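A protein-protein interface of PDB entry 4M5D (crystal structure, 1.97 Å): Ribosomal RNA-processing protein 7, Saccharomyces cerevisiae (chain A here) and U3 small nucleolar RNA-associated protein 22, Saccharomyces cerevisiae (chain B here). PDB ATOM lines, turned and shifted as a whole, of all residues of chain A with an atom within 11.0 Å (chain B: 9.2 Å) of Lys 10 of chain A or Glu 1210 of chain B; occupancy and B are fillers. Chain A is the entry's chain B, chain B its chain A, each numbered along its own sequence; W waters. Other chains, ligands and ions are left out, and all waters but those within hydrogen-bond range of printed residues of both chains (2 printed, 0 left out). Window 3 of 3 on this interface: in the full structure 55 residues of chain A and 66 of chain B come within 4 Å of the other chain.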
ATOM      1  N   ILE A   3       6.922  -4.911 -23.587  1.00  0.00           N
ATOM      2  CA  ILE A   3       8.022  -5.432 -24.463  1.00  0.00           C
ATOM      3  C   ILE A   3       7.580  -5.512 -25.923  1.00  0.00           C
ATOM      4  O   ILE A   3       8.322  -5.127 -26.830  1.00  0.00           O
ATOM      5  CB  ILE A   3       8.539  -6.824 -23.984  1.00  0.00           C
ATOM      6  CG1 ILE A   3       9.039  -6.758 -22.533  1.00  0.00           C
ATOM      7  CG2 ILE A   3       9.625  -7.370 -24.926  1.00  0.00           C
ATOM      8  CD1 ILE A   3      10.129  -5.718 -22.272  1.00  0.00           C
ATOM      9  N   ASP A   5       5.683  -3.658 -27.340  1.00  0.00           N
ATOM     10  CA  ASP A   5       5.584  -2.290 -27.854  1.00  0.00           C
ATOM     11  C   ASP A   5       6.912  -1.680 -28.281  1.00  0.00           C
ATOM     12  O   ASP A   5       6.940  -0.544 -28.762  1.00  0.00           O
ATOM     13  CB  ASP A   5       4.907  -1.373 -26.828  1.00  0.00           C
ATOM     14  CG  ASP A   5       3.456  -1.734 -26.596  1.00  0.00           C
ATOM     15  OD1 ASP A   5       2.743  -2.027 -27.582  1.00  0.00           O
ATOM     16  OD2 ASP A   5       3.029  -1.734 -25.424  1.00  0.00           O
ATOM     17  N   ILE A   6       8.005  -2.421 -28.106  1.00  0.00           N
ATOM     18  CA  ILE A   6       9.324  -1.915 -28.478  1.00  0.00           C
ATOM     19  C   ILE A   6       9.657  -2.302 -29.923  1.00  0.00           C
ATOM     20  O   ILE A   6      10.054  -3.439 -30.210  1.00  0.00           O
ATOM     21  CB  ILE A   6      10.450  -2.386 -27.526  1.00  0.00           C
ATOM     22  CG1 ILE A   6       9.981  -2.401 -26.065  1.00  0.00           C
ATOM     23  CG2 ILE A   6      11.650  -1.472 -27.669  1.00  0.00           C
ATOM     24  CD1 ILE A   6      10.926  -3.132 -25.111  1.00  0.00           C
ATOM     25  N   SER A   7       9.499  -1.333 -30.816  1.00  0.00           N
ATOM     26  CA  SER A   7       9.724  -1.530 -32.235  1.00  0.00           C
ATOM     27  C   SER A   7      11.104  -1.020 -32.654  1.00  0.00           C
ATOM     28  O   SER A   7      11.668  -1.492 -33.636  1.00  0.00           O
ATOM     29  CB  SER A   7       8.631  -0.809 -33.023  1.00  0.00           C
ATOM     30  OG  SER A   7       8.685   0.581 -32.767  1.00  0.00           O
ATOM     31  N   ALA A   8      11.631  -0.043 -31.913  1.00  0.00           N
ATOM     32  CA  ALA A   8      12.968   0.490 -32.171  1.00  0.00           C
ATOM     33  C   ALA A   8      13.655   0.890 -30.872  1.00  0.00           C
ATOM     34  O   ALA A   8      13.000   1.334 -29.924  1.00  0.00           O
ATOM     35  CB  ALA A   8      12.911   1.673 -33.137  1.00  0.00           C
ATOM     36  N   MET A   9      14.973   0.710 -30.832  1.00  0.00           N
ATOM     37  CA  MET A   9      15.794   1.125 -29.706  1.00  0.00           C
ATOM     38  C   MET A   9      16.151   2.599 -29.854  1.00  0.00           C
ATOM     39  O   MET A   9      16.165   3.131 -30.969  1.00  0.00           O
ATOM     40  CB  MET A   9      17.077   0.286 -29.625  1.00  0.00           C
ATOM     41  CG  MET A   9      16.865  -1.223 -29.495  1.00  0.00           C
ATOM     42  SD  MET A   9      15.987  -1.732 -27.998  1.00  0.00           S
ATOM     43  CE  MET A   9      14.352  -1.964 -28.621  1.00  0.00           C
ATOM     44  N   LYS A  10      16.451   3.238 -28.724  1.00  0.00           N
ATOM     45  CA  LYS A  10      16.806   4.658 -28.660  1.00  0.00           C
ATOM     46  C   LYS A  10      17.956   5.064 -29.596  1.00  0.00           C
ATOM     47  O   LYS A  10      17.959   6.172 -30.128  1.00  0.00           O
ATOM     48  CB  LYS A  10      17.123   5.052 -27.211  1.00  0.00           C
ATOM     49  CG  LYS A  10      17.303   6.546 -26.987  1.00  0.00           C
ATOM     50  CD  LYS A  10      17.511   6.869 -25.512  1.00  0.00           C
ATOM     51  CE  LYS A  10      17.308   8.355 -25.235  1.00  0.00           C
ATOM     52  NZ  LYS A  10      15.904   8.786 -25.508  1.00  0.00           N
ATOM     53  N   ASN A  11      18.919   4.170 -29.807  1.00  0.00           N
ATOM     54  CA  ASN A  11      20.061   4.479 -30.674  1.00  0.00           C
ATOM     55  C   ASN A  11      19.775   4.357 -32.182  1.00  0.00           C
ATOM     56  O   ASN A  11      20.677   4.519 -33.007  1.00  0.00           O
ATOM     57  CB  ASN A  11      21.281   3.645 -30.274  1.00  0.00           C
ATOM     58  CG  ASN A  11      21.040   2.134 -30.394  1.00  0.00           C
ATOM     59  OD1 ASN A  11      19.956   1.677 -30.769  1.00  0.00           O
ATOM     60  ND2 ASN A  11      22.063   1.359 -30.073  1.00  0.00           N
ATOM     61  N   GLY A  12      18.523   4.071 -32.536  1.00  0.00           N
ATOM     62  CA  GLY A  12      18.110   4.022 -33.940  1.00  0.00           C
ATOM     63  C   GLY A  12      17.999   2.630 -34.547  1.00  0.00           C
ATOM     64  O   GLY A  12      17.681   2.493 -35.737  1.00  0.00           O
ATOM     65  N   PHE A  13      18.260   1.598 -33.739  1.00  0.00           N
ATOM     66  CA  PHE A  13      18.160   0.215 -34.204  1.00  0.00           C
ATOM     67  C   PHE A  13      16.722  -0.286 -34.160  1.00  0.00           C
ATOM     68  O   PHE A  13      16.079  -0.264 -33.109  1.00  0.00           O
ATOM     69  CB  PHE A  13      19.068  -0.717 -33.388  1.00  0.00           C
ATOM     70  CG  PHE A  13      20.505  -0.731 -33.850  1.00  0.00           C
ATOM     71  CD1 PHE A  13      21.430   0.159 -33.317  1.00  0.00           C
ATOM     72  CD2 PHE A  13      20.927  -1.633 -34.815  1.00  0.00           C
ATOM     73  CE1 PHE A  13      22.759   0.153 -33.743  1.00  0.00           C
ATOM     74  CE2 PHE A  13      22.253  -1.650 -35.246  1.00  0.00           C
ATOM     75  CZ  PHE A  13      23.168  -0.750 -34.708  1.00  0.00           C
ATOM     76  N   ILE A  14      16.233  -0.746 -35.308  1.00  0.00           N
ATOM     77  CA  ILE A  14      14.922  -1.389 -35.397  1.00  0.00           C
ATOM     78  C   ILE A  14      15.020  -2.795 -34.812  1.00  0.00           C
ATOM     79  O   ILE A  14      16.002  -3.504 -35.050  1.00  0.00           O
ATOM     80  CB  ILE A  14      14.431  -1.480 -36.867  1.00  0.00           C
ATOM     81  CG1 ILE A  14      14.021  -0.105 -37.401  1.00  0.00           C
ATOM     82  CG2 ILE A  14      13.256  -2.463 -37.001  1.00  0.00           C
ATOM     83  CD1 ILE A  14      13.425  -0.172 -38.819  1.00  0.00           C
ATOM     84  N   VAL A  15      13.996  -3.193 -34.070  1.00  0.00           N
ATOM     85  CA  VAL A  15      13.934  -4.533 -33.485  1.00  0.00           C
ATOM     86  C   VAL A  15      13.208  -5.505 -34.426  1.00  0.00           C
ATOM     87  O   VAL A  15      12.046  -5.295 -34.800  1.00  0.00           O
ATOM     88  CB  VAL A  15      13.295  -4.490 -32.081  1.00  0.00           C
ATOM     89  CG1 VAL A  15      13.236  -5.875 -31.443  1.00  0.00           C
ATOM     90  CG2 VAL A  15      14.080  -3.528 -31.202  1.00  0.00           C
ATOM     91  N   PHE A  38      18.735  -6.913 -34.537  1.00  0.00           N
ATOM     92  CA  PHE A  38      18.668  -5.453 -34.558  1.00  0.00           C
ATOM     93  C   PHE A  38      19.287  -4.915 -35.843  1.00  0.00           C
ATOM     94  O   PHE A  38      20.342  -5.393 -36.282  1.00  0.00           O
ATOM     95  CB  PHE A  38      19.398  -4.867 -33.344  1.00  0.00           C
ATOM     96  CG  PHE A  38      18.861  -5.342 -32.014  1.00  0.00           C
ATOM     97  CD1 PHE A  38      19.298  -6.545 -31.456  1.00  0.00           C
ATOM     98  CD2 PHE A  38      17.937  -4.573 -31.306  1.00  0.00           C
ATOM     99  CE1 PHE A  38      18.806  -6.992 -30.215  1.00  0.00           C
ATOM    100  CE2 PHE A  38      17.437  -5.008 -30.064  1.00  0.00           C
ATOM    101  CZ  PHE A  38      17.877  -6.225 -29.519  1.00  0.00           C
ATOM    102  N   ALA A  39      18.637  -3.915 -36.444  1.00  0.00           N
ATOM    103  CA  ALA A  39      19.045  -3.409 -37.754  1.00  0.00           C
ATOM    104  C   ALA A  39      19.057  -1.879 -37.822  1.00  0.00           C
ATOM    105  O   ALA A  39      18.151  -1.212 -37.304  1.00  0.00           O
ATOM    106  CB  ALA A  39      18.127  -3.982 -38.845  1.00  0.00           C
ATOM    107  N   LYS A  40      20.079  -1.334 -38.476  1.00  0.00           N
ATOM    108  CA  LYS A  40      20.186   0.104 -38.716  1.00  0.00           C
ATOM    109  C   LYS A  40      20.872   0.328 -40.061  1.00  0.00           C
ATOM    110  O   LYS A  40      21.692  -0.496 -40.477  1.00  0.00           O
ATOM    111  CB  LYS A  40      21.008   0.755 -37.609  1.00  0.00           C
ATOM    112  CG  LYS A  40      20.871   2.259 -37.509  1.00  0.00           C
ATOM    113  CD  LYS A  40      21.735   2.781 -36.377  1.00  0.00           C
ATOM    114  CE  LYS A  40      21.586   4.274 -36.215  1.00  0.00           C
ATOM    115  NZ  LYS A  40      22.410   4.736 -35.073  1.00  0.00           N
ATOM    116  N   TRP A 138      14.139  -1.440 -45.882  1.00  0.00           N
ATOM    117  CA  TRP A 138      14.120  -0.658 -44.650  1.00  0.00           C
ATOM    118  C   TRP A 138      12.703  -0.226 -44.291  1.00  0.00           C
ATOM    119  O   TRP A 138      12.307  -0.290 -43.122  1.00  0.00           O
ATOM    120  CB  TRP A 138      15.036   0.556 -44.765  1.00  0.00           C
ATOM    121  CG  TRP A 138      15.032   1.433 -43.550  1.00  0.00           C
ATOM    122  CD1 TRP A 138      14.431   2.653 -43.423  1.00  0.00           C
ATOM    123  CD2 TRP A 138      15.649   1.156 -42.284  1.00  0.00           C
ATOM    124  NE1 TRP A 138      14.647   3.159 -42.166  1.00  0.00           N
ATOM    125  CE2 TRP A 138      15.390   2.262 -41.445  1.00  0.00           C
ATOM    126  CE3 TRP A 138      16.400   0.082 -41.781  1.00  0.00           C
ATOM    127  CZ2 TRP A 138      15.858   2.330 -40.124  1.00  0.00           C
ATOM    128  CZ3 TRP A 138      16.866   0.148 -40.470  1.00  0.00           C
ATOM    129  CH2 TRP A 138      16.594   1.267 -39.657  1.00  0.00           C
ATOM    130  N   ALA B1193      20.845  -6.880 -16.607  1.00  0.00           N
ATOM    131  CA  ALA B1193      20.628  -6.051 -17.792  1.00  0.00           C
ATOM    132  C   ALA B1193      21.814  -5.133 -18.081  1.00  0.00           C
ATOM    133  O   ALA B1193      22.594  -4.826 -17.187  1.00  0.00           O
ATOM    134  CB  ALA B1193      19.355  -5.241 -17.636  1.00  0.00           C
ATOM    135  N   HIS B1194      21.946  -4.714 -19.335  1.00  0.00           N
ATOM    136  CA  HIS B1194      22.988  -3.771 -19.759  1.00  0.00           C
ATOM    137  C   HIS B1194      22.436  -2.809 -20.796  1.00  0.00           C
ATOM    138  O   HIS B1194      21.443  -3.109 -21.453  1.00  0.00           O
ATOM    139  CB  HIS B1194      24.195  -4.507 -20.357  1.00  0.00           C
ATOM    140  CG  HIS B1194      24.854  -5.464 -19.412  1.00  0.00           C
ATOM    141  ND1 HIS B1194      25.547  -5.050 -18.293  1.00  0.00           N
ATOM    142  CD2 HIS B1194      24.919  -6.817 -19.416  1.00  0.00           C
ATOM    143  CE1 HIS B1194      26.010  -6.107 -17.647  1.00  0.00           C
ATOM    144  NE2 HIS B1194      25.644  -7.191 -18.310  1.00  0.00           N
ATOM    145  N   LYS B1195      23.076  -1.651 -20.932  1.00  0.00           N
ATOM    146  CA  LYS B1195      22.821  -0.749 -22.053  1.00  0.00           C
ATOM    147  C   LYS B1195      23.035  -1.486 -23.361  1.00  0.00           C
ATOM    148  O   LYS B1195      24.002  -2.244 -23.507  1.00  0.00           O
ATOM    149  CB  LYS B1195      23.761   0.462 -22.026  1.00  0.00           C
ATOM    150  CG  LYS B1195      23.462   1.482 -20.949  1.00  0.00           C
ATOM    151  CD  LYS B1195      22.203   2.274 -21.269  1.00  0.00           C
ATOM    152  CE  LYS B1195      21.637   2.918 -20.016  1.00  0.00           C
ATOM    153  NZ  LYS B1195      21.209   1.893 -19.020  1.00  0.00           N
ATOM    154  N   PHE B1196      22.130  -1.262 -24.309  1.00  0.00           N
ATOM    155  CA  PHE B1196      22.290  -1.801 -25.650  1.00  0.00           C
ATOM    156  C   PHE B1196      23.491  -1.129 -26.326  1.00  0.00           C
ATOM    157  O   PHE B1196      23.508   0.091 -26.493  1.00  0.00           O
ATOM    158  CB  PHE B1196      20.999  -1.626 -26.469  1.00  0.00           C
ATOM    159  CG  PHE B1196      21.074  -2.207 -27.858  1.00  0.00           C
ATOM    160  CD1 PHE B1196      21.075  -3.584 -28.058  1.00  0.00           C
ATOM    161  CD2 PHE B1196      21.147  -1.379 -28.965  1.00  0.00           C
ATOM    162  CE1 PHE B1196      21.151  -4.124 -29.344  1.00  0.00           C
ATOM    163  CE2 PHE B1196      21.227  -1.913 -30.257  1.00  0.00           C
ATOM    164  CZ  PHE B1196      21.226  -3.291 -30.439  1.00  0.00           C
ATOM    165  N   ARG B1197      24.502  -1.931 -26.658  1.00  0.00           N
ATOM    166  CA  ARG B1197      25.690  -1.475 -27.395  1.00  0.00           C
ATOM    167  C   ARG B1197      25.924  -2.422 -28.563  1.00  0.00           C
ATOM    168  O   ARG B1197      25.622  -3.610 -28.458  1.00  0.00           O
ATOM    169  CB  ARG B1197      26.943  -1.518 -26.513  1.00  0.00           C
ATOM    170  CG  ARG B1197      26.831  -0.848 -25.172  1.00  0.00           C
ATOM    171  CD  ARG B1197      28.028  -1.201 -24.300  1.00  0.00           C
ATOM    172  NE  ARG B1197      28.047  -0.391 -23.085  1.00  0.00           N
ATOM    173  CZ  ARG B1197      27.385  -0.690 -21.969  1.00  0.00           C
ATOM    174  NH1 ARG B1197      26.643  -1.792 -21.900  1.00  0.00           N
ATOM    175  NH2 ARG B1197      27.466   0.120 -20.918  1.00  0.00           N
ATOM    176  N   LEU B1200      28.235  -5.708 -27.657  1.00  0.00           N
ATOM    177  CA  LEU B1200      27.894  -6.526 -26.501  1.00  0.00           C
ATOM    178  C   LEU B1200      28.200  -8.023 -26.683  1.00  0.00           C
ATOM    179  O   LEU B1200      28.465  -8.721 -25.710  1.00  0.00           O
ATOM    180  CB  LEU B1200      26.428  -6.322 -26.132  1.00  0.00           C
ATOM    181  CG  LEU B1200      26.040  -6.573 -24.676  1.00  0.00           C
ATOM    182  CD1 LEU B1200      26.714  -5.555 -23.742  1.00  0.00           C
ATOM    183  CD2 LEU B1200      24.539  -6.506 -24.522  1.00  0.00           C
ATOM    184  N   LYS B1205      17.634  -9.842 -25.607  1.00  0.00           N
ATOM    185  CA  LYS B1205      16.298  -9.307 -25.893  1.00  0.00           C
ATOM    186  C   LYS B1205      16.151  -7.931 -25.218  1.00  0.00           C
ATOM    187  O   LYS B1205      16.766  -7.691 -24.165  1.00  0.00           O
ATOM    188  CB  LYS B1205      15.212 -10.272 -25.403  1.00  0.00           C
ATOM    189  CG  LYS B1205      15.238 -10.558 -23.905  1.00  0.00           C
ATOM    190  CD  LYS B1205      14.243 -11.630 -23.524  1.00  0.00           C
ATOM    191  CE  LYS B1205      14.146 -11.759 -22.018  1.00  0.00           C
ATOM    192  NZ  LYS B1205      13.229 -12.869 -21.644  1.00  0.00           N
ATOM    193  N   PRO B1206      15.348  -7.018 -25.814  1.00  0.00           N
ATOM    194  CA  PRO B1206      15.175  -5.718 -25.158  1.00  0.00           C
ATOM    195  C   PRO B1206      14.376  -5.848 -23.857  1.00  0.00           C
ATOM    196  O   PRO B1206      13.495  -6.697 -23.763  1.00  0.00           O
ATOM    197  CB  PRO B1206      14.388  -4.882 -26.186  1.00  0.00           C
ATOM    198  CG  PRO B1206      14.353  -5.689 -27.453  1.00  0.00           C
ATOM    199  CD  PRO B1206      14.575  -7.126 -27.066  1.00  0.00           C
ATOM    200  N   VAL B1207      14.696  -5.028 -22.860  1.00  0.00           N
ATOM    201  CA  VAL B1207      13.835  -4.908 -21.664  1.00  0.00           C
ATOM    202  C   VAL B1207      13.134  -3.547 -21.658  1.00  0.00           C
ATOM    203  O   VAL B1207      12.121  -3.365 -20.995  1.00  0.00           O
ATOM    204  CB  VAL B1207      14.588  -5.162 -20.331  1.00  0.00           C
ATOM    205  CG1 VAL B1207      15.109  -6.609 -20.280  1.00  0.00           C
ATOM    206  CG2 VAL B1207      15.715  -4.150 -20.122  1.00  0.00           C
ATOM    207  N   ASP B1208      13.700  -2.611 -22.410  1.00  0.00           N
ATOM    208  CA  ASP B1208      13.069  -1.341 -22.769  1.00  0.00           C
ATOM    209  C   ASP B1208      13.791  -0.850 -24.024  1.00  0.00           C
ATOM    210  O   ASP B1208      14.501  -1.632 -24.664  1.00  0.00           O
ATOM    211  CB  ASP B1208      13.138  -0.322 -21.618  1.00  0.00           C
ATOM    212  CG  ASP B1208      14.520  -0.208 -21.012  1.00  0.00           C
ATOM    213  OD1 ASP B1208      15.511  -0.042 -21.756  1.00  0.00           O
ATOM    214  OD2 ASP B1208      14.609  -0.274 -19.771  1.00  0.00           O
ATOM    215  N   ASP B1209      13.640   0.424 -24.376  1.00  0.00           N
ATOM    216  CA  ASP B1209      14.241   0.944 -25.610  1.00  0.00           C
ATOM    217  C   ASP B1209      15.736   1.295 -25.490  1.00  0.00           C
ATOM    218  O   ASP B1209      16.375   1.689 -26.480  1.00  0.00           O
ATOM    219  CB  ASP B1209      13.431   2.136 -26.147  1.00  0.00           C
ATOM    220  CG  ASP B1209      13.631   3.407 -25.326  1.00  0.00           C
ATOM    221  OD1 ASP B1209      13.823   3.306 -24.093  1.00  0.00           O
ATOM    222  OD2 ASP B1209      13.591   4.507 -25.921  1.00  0.00           O
ATOM    223  N   GLU B1210      16.291   1.136 -24.289  1.00  0.00           N
ATOM    224  CA  GLU B1210      17.694   1.474 -24.027  1.00  0.00           C
ATOM    225  C   GLU B1210      18.541   0.306 -23.529  1.00  0.00           C
ATOM    226  O   GLU B1210      19.773   0.318 -23.675  1.00  0.00           O
ATOM    227  CB  GLU B1210      17.778   2.610 -23.008  1.00  0.00           C
ATOM    228  CG  GLU B1210      17.167   3.914 -23.483  1.00  0.00           C
ATOM    229  CD  GLU B1210      17.077   4.935 -22.374  1.00  0.00           C
ATOM    230  OE1 GLU B1210      18.115   5.214 -21.735  1.00  0.00           O
ATOM    231  OE2 GLU B1210      15.966   5.456 -22.138  1.00  0.00           O
ATOM    232  N   ASN B1211      17.881  -0.685 -22.935  1.00  0.00           N
ATOM    233  CA  ASN B1211      18.568  -1.774 -22.250  1.00  0.00           C
ATOM    234  C   ASN B1211      18.142  -3.149 -22.726  1.00  0.00           C
ATOM    235  O   ASN B1211      17.008  -3.345 -23.177  1.00  0.00           O
ATOM    236  CB  ASN B1211      18.358  -1.663 -20.743  1.00  0.00           C
ATOM    237  CG  ASN B1211      18.810  -0.323 -20.200  1.00  0.00           C
ATOM    238  OD1 ASN B1211      20.000  -0.032 -20.164  1.00  0.00           O
ATOM    239  ND2 ASN B1211      17.859   0.506 -19.802  1.00  0.00           N
ATOM    240  N   VAL B1212      19.062  -4.102 -22.601  1.00  0.00           N
ATOM    241  CA  VAL B1212      18.828  -5.472 -23.035  1.00  0.00           C
ATOM    242  C   VAL B1212      19.309  -6.483 -22.005  1.00  0.00           C
ATOM    243  O   VAL B1212      20.084  -6.155 -21.096  1.00  0.00           O
ATOM    244  CB  VAL B1212      19.509  -5.764 -24.401  1.00  0.00           C
ATOM    245  CG1 VAL B1212      18.855  -4.946 -25.512  1.00  0.00           C
ATOM    246  CG2 VAL B1212      21.015  -5.490 -24.333  1.00  0.00           C
ATOM    247  N   ILE B1213      18.851  -7.718 -22.156  1.00  0.00           N
ATOM    248  CA  ILE B1213      19.248  -8.792 -21.260  1.00  0.00           C
ATOM    249  C   ILE B1213      19.474 -10.067 -22.072  1.00  0.00           C
ATOM    250  O   ILE B1213      18.808 -10.283 -23.093  1.00  0.00           O
ATOM    251  CB  ILE B1213      18.192  -8.974 -20.132  1.00  0.00           C
ATOM    252  CG1 ILE B1213      18.837  -9.527 -18.858  1.00  0.00           C
ATOM    253  CG2 ILE B1213      16.979  -9.786 -20.609  1.00  0.00           C
ATOM    254  CD1 ILE B1213      17.934  -9.457 -17.609  1.00  0.00           C
HETATM  255  O   HOH W   1      13.021   4.355 -29.163  1.00  0.00           O
HETATM  256  O   HOH W   2      19.124   2.018 -27.567  1.00  0.00           O
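The backbone carbonyl oxygen (O) of Asp 1209 of chain B is in hydrogen-bond range of the backbone NH (N) of Lys 10 of chain A (2.7 Å).
The backbone carbonyl oxygen (O) of Asp 1208 of chain B lies close to the side-chain sulfur (SD) of Met 9 of chain A (3.7 Å).
The side-chain sulfur of Met 9 of chain A lies close to the backbone carbonyl oxygen of Asp 1209 of chain B (3.8 Å).
Water W2 lies within hydrogen-bond range of the backbone carbonyl oxygen of Asp 1209 of chain B (3.0 Å), the backbone NH of Asn 11 of chain A (3.1 Å) and the backbone NH of Lys 10 of chain A (3.2 Å).
Water W1 bridges O of Ala 8 of chain A (3.1 Å) and OD2 of Asp 1209 of chain B (3.3 Å).
Of the printed residues of chain B, Met 9 of chain A touches Pro 1206 (3.8 Å), Asp 1208 (3.7 Å) and Asp 1209 (3.3 Å).
Lys 10 of chain A touches just these residues of chain B: Asp 1209 (2.7 Å) and Glu 1210 (3.6 Å).
Printed residues of chain B within 4 Å of Asn 11 of chain A: Phe 1196.
Ile 14 of chain A touches none of the printed residues of chain B.
Trp 138 of chain A touches none of the printed residues of chain B.
No residue of chain A comes within 4 Å of Lys 1195 of chain B.
Of the printed residues of chain A, Phe 1196 of chain B touches Asn 11 (3.1 Å), Phe 13 (3.7 Å) and Phe 38 (3.5 Å).
Of the printed residues of chain A, Pro 1206 of chain B touches Ile 3 (3.8 Å) and Met 9 (3.8 Å).
Of chain A, only Ala 8 (3.9 Å), Met 9 (3.3 Å) and Lys 10 (2.7 Å) come within 4 Å of Asp 1209 of chain B.
Glu 1210 of chain B touches just one residue of chain A: Lys 10 (3.6 Å).
The nearest printed residue of chain A that does not touch Val 1207 of chain B is Ile 6 of chain A (4.1 Å).
O of Glu 1210 of chain B is in hydrogen-bond range of N of Phe 1196 of chain B, 2.9 Å away.
N of Glu 1210 of chain B lies within hydrogen-bond range of OD1 of Asp 1208 of chain B.
The backbone NH (N) of Asn 1211 of chain B is in hydrogen-bond range of the side-chain carboxylate (OD1) of Asp 1208 of chain B (2.7 Å).
The side-chain amide oxygen (OD1) of Asn 11 of chain A sits close to the backbone NH (N) of Phe 13 of chain A, 3.4 Å away.
The side-chain amino group of Lys 40 of chain A sits at hydrogen-bond distance from the backbone carbonyl oxygen of Asn 11 of chain A (2.7 Å).
Hydrophobic or aromatic side chains of chain B that line the printed part of chain A: Phe 1196 and Pro 1206.
Hydrophobic or aromatic side chains of chain A that line the printed part of chain B: Ile 3, Ile 6, Met 9, Phe 13 and Phe 38.
Among the printed residues, no Asp or Glu carboxylate lies within 4 Å of a Lys or Arg side-chain nitrogen of the other chain.
Pro 1206 of chain B touches Ile 3 of chain A (O to CD1, 3.8 Å).
Ile 3 of chain A touches Val 1207 of chain B (CD1 to O, 3.3 Å).
CD1 of Ile 6 of chain A touches CA of Asp 1208 of chain B, at 3.6 Å.
Asp 1209 of chain B touches Ala 8 of chain A.
Met 9 of chain A touches Pro 1206 of chain B (CE to CB, 3.8 Å).
CD of Lys 10 of chain A touches CG of Glu 1210 of chain B (3.6 Å).
Phe 1196 of chain B touches Asn 11 of chain A (CD2 to ND2, 3.1 Å).
CD1 of Phe 13 of chain A touches CE2 of Phe 1196 of chain B, at 3.7 Å.
Phe 38 of chain A touches Phe 1196 of chain B (CG to CZ, 3.5 Å).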
